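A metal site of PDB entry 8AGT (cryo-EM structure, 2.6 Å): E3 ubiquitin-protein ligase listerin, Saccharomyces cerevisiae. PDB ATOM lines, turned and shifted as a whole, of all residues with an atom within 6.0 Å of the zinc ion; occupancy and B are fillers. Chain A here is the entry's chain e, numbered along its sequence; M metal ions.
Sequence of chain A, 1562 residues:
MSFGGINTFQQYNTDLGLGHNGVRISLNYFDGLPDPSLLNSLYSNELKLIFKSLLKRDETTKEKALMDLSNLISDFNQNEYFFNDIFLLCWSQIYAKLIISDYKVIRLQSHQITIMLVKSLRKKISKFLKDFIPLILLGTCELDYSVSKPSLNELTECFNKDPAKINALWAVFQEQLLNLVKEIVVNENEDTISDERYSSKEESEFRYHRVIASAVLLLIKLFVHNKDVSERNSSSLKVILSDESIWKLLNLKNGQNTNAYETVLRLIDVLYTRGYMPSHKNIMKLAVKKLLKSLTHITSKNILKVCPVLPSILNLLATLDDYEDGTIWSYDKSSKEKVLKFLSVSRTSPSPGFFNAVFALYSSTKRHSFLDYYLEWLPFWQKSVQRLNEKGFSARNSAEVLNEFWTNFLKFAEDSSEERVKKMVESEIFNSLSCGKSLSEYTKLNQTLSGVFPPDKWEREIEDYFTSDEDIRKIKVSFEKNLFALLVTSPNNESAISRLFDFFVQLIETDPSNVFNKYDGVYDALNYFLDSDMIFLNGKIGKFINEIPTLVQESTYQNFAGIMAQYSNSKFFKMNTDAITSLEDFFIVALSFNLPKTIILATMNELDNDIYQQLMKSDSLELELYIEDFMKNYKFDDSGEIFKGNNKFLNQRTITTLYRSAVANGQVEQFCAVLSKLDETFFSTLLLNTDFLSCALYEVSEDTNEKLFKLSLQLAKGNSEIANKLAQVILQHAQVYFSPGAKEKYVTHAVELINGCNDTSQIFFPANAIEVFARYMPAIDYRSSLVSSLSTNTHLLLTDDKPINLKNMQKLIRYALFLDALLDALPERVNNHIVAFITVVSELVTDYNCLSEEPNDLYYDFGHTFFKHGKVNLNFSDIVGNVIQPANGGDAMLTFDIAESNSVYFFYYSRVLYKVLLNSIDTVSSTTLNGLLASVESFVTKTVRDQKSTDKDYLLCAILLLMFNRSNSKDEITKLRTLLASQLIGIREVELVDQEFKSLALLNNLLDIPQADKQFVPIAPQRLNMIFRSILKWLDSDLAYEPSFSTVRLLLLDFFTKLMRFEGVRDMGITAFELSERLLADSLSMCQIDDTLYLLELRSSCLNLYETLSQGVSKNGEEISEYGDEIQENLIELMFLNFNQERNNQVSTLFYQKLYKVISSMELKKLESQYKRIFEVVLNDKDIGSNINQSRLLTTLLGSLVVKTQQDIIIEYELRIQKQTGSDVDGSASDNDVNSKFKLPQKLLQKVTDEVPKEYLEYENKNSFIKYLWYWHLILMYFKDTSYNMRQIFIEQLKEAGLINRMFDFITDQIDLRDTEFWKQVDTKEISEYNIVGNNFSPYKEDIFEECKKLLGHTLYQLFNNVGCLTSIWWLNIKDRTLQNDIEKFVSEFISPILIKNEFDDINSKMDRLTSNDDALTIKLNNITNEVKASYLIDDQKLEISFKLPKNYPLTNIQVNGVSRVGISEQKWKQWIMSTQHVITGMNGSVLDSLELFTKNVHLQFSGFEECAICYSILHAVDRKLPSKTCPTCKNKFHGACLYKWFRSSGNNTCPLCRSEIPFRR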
ATOM      1  N   CYS A1508     -26.762  -8.514 -19.438  1.00  0.00           N
ATOM      2  CA  CYS A1508     -27.367  -7.961 -18.237  1.00  0.00           C
ATOM      3  C   CYS A1508     -26.915  -6.516 -18.154  1.00  0.00           C
ATOM      4  O   CYS A1508     -25.742  -6.223 -18.364  1.00  0.00           O
ATOM      5  CB  CYS A1508     -26.930  -8.736 -16.998  1.00  0.00           C
ATOM      6  SG  CYS A1508     -26.388  -7.738 -15.589  1.00  0.00           S
ATOM      7  N   ALA A1509     -27.823  -5.597 -17.840  1.00  0.00           N
ATOM      8  CA  ALA A1509     -27.472  -4.178 -17.838  1.00  0.00           C
ATOM      9  C   ALA A1509     -26.431  -3.762 -16.806  1.00  0.00           C
ATOM     10  O   ALA A1509     -25.564  -2.940 -17.113  1.00  0.00           O
ATOM     11  CB  ALA A1509     -28.728  -3.328 -17.696  1.00  0.00           C
ATOM     12  N   ILE A1510     -26.509  -4.297 -15.596  1.00  0.00           N
ATOM     13  CA  ILE A1510     -25.591  -3.862 -14.545  1.00  0.00           C
ATOM     14  C   ILE A1510     -24.112  -4.143 -14.842  1.00  0.00           C
ATOM     15  O   ILE A1510     -23.269  -3.269 -14.639  1.00  0.00           O
ATOM     16  CB  ILE A1510     -25.964  -4.522 -13.200  1.00  0.00           C
ATOM     17  CG1 ILE A1510     -27.479  -4.522 -13.014  1.00  0.00           C
ATOM     18  CG2 ILE A1510     -25.272  -3.828 -12.032  1.00  0.00           C
ATOM     19  CD1 ILE A1510     -27.938  -5.237 -11.768  1.00  0.00           C
ATOM     20  N   CYS A1511     -23.804  -5.337 -15.328  1.00  0.00           N
ATOM     21  CA  CYS A1511     -22.410  -5.681 -15.641  1.00  0.00           C
ATOM     22  C   CYS A1511     -22.089  -5.659 -17.129  1.00  0.00           C
ATOM     23  O   CYS A1511     -20.951  -5.932 -17.512  1.00  0.00           O
ATOM     24  CB  CYS A1511     -22.052  -7.034 -15.034  1.00  0.00           C
ATOM     25  SG  CYS A1511     -23.275  -8.321 -15.338  1.00  0.00           S
ATOM     26  N   TYR A1512     -23.080  -5.368 -17.967  1.00  0.00           N
ATOM     27  CA  TYR A1512     -22.884  -5.302 -19.423  1.00  0.00           C
ATOM     28  C   TYR A1512     -22.301  -6.601 -20.011  1.00  0.00           C
ATOM     29  O   TYR A1512     -21.486  -6.555 -20.924  1.00  0.00           O
ATOM     30  CB  TYR A1512     -22.039  -4.086 -19.815  1.00  0.00           C
ATOM     31  CG  TYR A1512     -22.350  -3.522 -21.180  1.00  0.00           C
ATOM     32  CD1 TYR A1512     -23.634  -3.067 -21.485  1.00  0.00           C
ATOM     33  CD2 TYR A1512     -21.376  -3.434 -22.166  1.00  0.00           C
ATOM     34  CE1 TYR A1512     -23.928  -2.557 -22.735  1.00  0.00           C
ATOM     35  CE2 TYR A1512     -21.661  -2.925 -23.413  1.00  0.00           C
ATOM     36  CZ  TYR A1512     -22.933  -2.487 -23.696  1.00  0.00           C
ATOM     37  OH  TYR A1512     -23.230  -1.973 -24.937  1.00  0.00           O
ATOM     38  N   SER A1513     -22.731  -7.739 -19.483  1.00  0.00           N
ATOM     39  CA  SER A1513     -22.251  -9.016 -19.992  1.00  0.00           C
ATOM     40  C   SER A1513     -23.376 -10.024 -20.152  1.00  0.00           C
ATOM     41  O   SER A1513     -24.264 -10.098 -19.310  1.00  0.00           O
ATOM     42  CB  SER A1513     -21.169  -9.591 -19.085  1.00  0.00           C
ATOM     43  OG  SER A1513     -21.675  -9.834 -17.782  1.00  0.00           O
ATOM     44  N   HIS A1516     -22.608 -14.004 -16.605  1.00  0.00           N
ATOM     45  CA  HIS A1516     -22.082 -13.495 -15.347  1.00  0.00           C
ATOM     46  C   HIS A1516     -20.664 -14.027 -15.248  1.00  0.00           C
ATOM     47  O   HIS A1516     -20.428 -15.189 -15.535  1.00  0.00           O
ATOM     48  CB  HIS A1516     -22.920 -14.014 -14.190  1.00  0.00           C
ATOM     49  CG  HIS A1516     -22.736 -13.251 -12.908  1.00  0.00           C
ATOM     50  ND1 HIS A1516     -21.659 -13.444 -12.077  1.00  0.00           N
ATOM     51  CD2 HIS A1516     -23.508 -12.308 -12.321  1.00  0.00           C
ATOM     52  CE1 HIS A1516     -21.770 -12.651 -11.029  1.00  0.00           C
ATOM     53  NE2 HIS A1516     -22.877 -11.952 -11.150  1.00  0.00           N
ATOM     54  N   PHE A1534     -31.109  -8.672 -16.483  1.00  0.00           N
ATOM     55  CA  PHE A1534     -30.234  -8.559 -15.330  1.00  0.00           C
ATOM     56  C   PHE A1534     -29.924  -9.948 -14.803  1.00  0.00           C
ATOM     57  O   PHE A1534     -30.816 -10.782 -14.691  1.00  0.00           O
ATOM     58  CB  PHE A1534     -30.921  -7.780 -14.206  1.00  0.00           C
ATOM     59  CG  PHE A1534     -31.437  -6.434 -14.620  1.00  0.00           C
ATOM     60  CD1 PHE A1534     -30.574  -5.353 -14.743  1.00  0.00           C
ATOM     61  CD2 PHE A1534     -32.782  -6.238 -14.873  1.00  0.00           C
ATOM     62  CE1 PHE A1534     -31.052  -4.119 -15.114  1.00  0.00           C
ATOM     63  CE2 PHE A1534     -33.266  -5.005 -15.256  1.00  0.00           C
ATOM     64  CZ  PHE A1534     -32.396  -3.935 -15.373  1.00  0.00           C
ATOM     65  N   HIS A1535     -28.661 -10.205 -14.489  1.00  0.00           N
ATOM     66  CA  HIS A1535     -28.317 -11.493 -13.887  1.00  0.00           C
ATOM     67  C   HIS A1535     -29.006 -11.583 -12.546  1.00  0.00           C
ATOM     68  O   HIS A1535     -29.129 -10.575 -11.850  1.00  0.00           O
ATOM     69  CB  HIS A1535     -26.820 -11.650 -13.686  1.00  0.00           C
ATOM     70  CG  HIS A1535     -26.043 -11.748 -14.961  1.00  0.00           C
ATOM     71  ND1 HIS A1535     -25.119 -10.809 -15.337  1.00  0.00           N
ATOM     72  CD2 HIS A1535     -26.062 -12.678 -15.947  1.00  0.00           C
ATOM     73  CE1 HIS A1535     -24.594 -11.156 -16.506  1.00  0.00           C
ATOM     74  NE2 HIS A1535     -25.164 -12.287 -16.891  1.00  0.00           N
ATOM     75  N   CYS A1538     -26.753 -10.366  -9.793  1.00  0.00           N
ATOM     76  CA  CYS A1538     -26.580  -8.919  -9.851  1.00  0.00           C
ATOM     77  C   CYS A1538     -27.841  -8.229  -9.361  1.00  0.00           C
ATOM     78  O   CYS A1538     -27.781  -7.277  -8.593  1.00  0.00           O
ATOM     79  CB  CYS A1538     -26.295  -8.473 -11.293  1.00  0.00           C
ATOM     80  SG  CYS A1538     -24.715  -9.003 -12.000  1.00  0.00           S
HETATM   81 ZN    ZN M   1     -24.847  -8.991 -14.344  1.00  0.00          ZN
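The side-chain sulfur (SG) of Cys 1511 lies close to the side-chain hydroxyl (OG) of Ser 1513, at 3.3 Å.
N of His 1516 sits at hydrogen-bond distance from NE2 of His 1535.
O of Ser 1513 sits close to NE2 of His 1535.
SG of Cys 1508 sits close to N of Ile 1510, at 3.4 Å.
The backbone NH (N) of Cys 1508 lies within hydrogen-bond range of the backbone carbonyl oxygen (O) of Ser 1513, 3.0 Å away.
NE2 of His 1516 lies close to SG of Cys 1538 (3.6 Å).
Within 4 Å of the zinc ion: Cys 1508, Cys 1511, His 1535 and Cys 1538.
The nearest printed residue that does not touch the zinc ion is His 1516 (4.1 Å).
SG of Cys 1511 is bound to the zinc ion (2.0 Å).
The zinc ion is bound by a ring nitrogen (ND1) of His 1535, 2.1 Å away.
SG of Cys 1508 binds the zinc ion (2.3 Å).
SG of Cys 1538 is bound to the zinc ion (2.3 Å).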
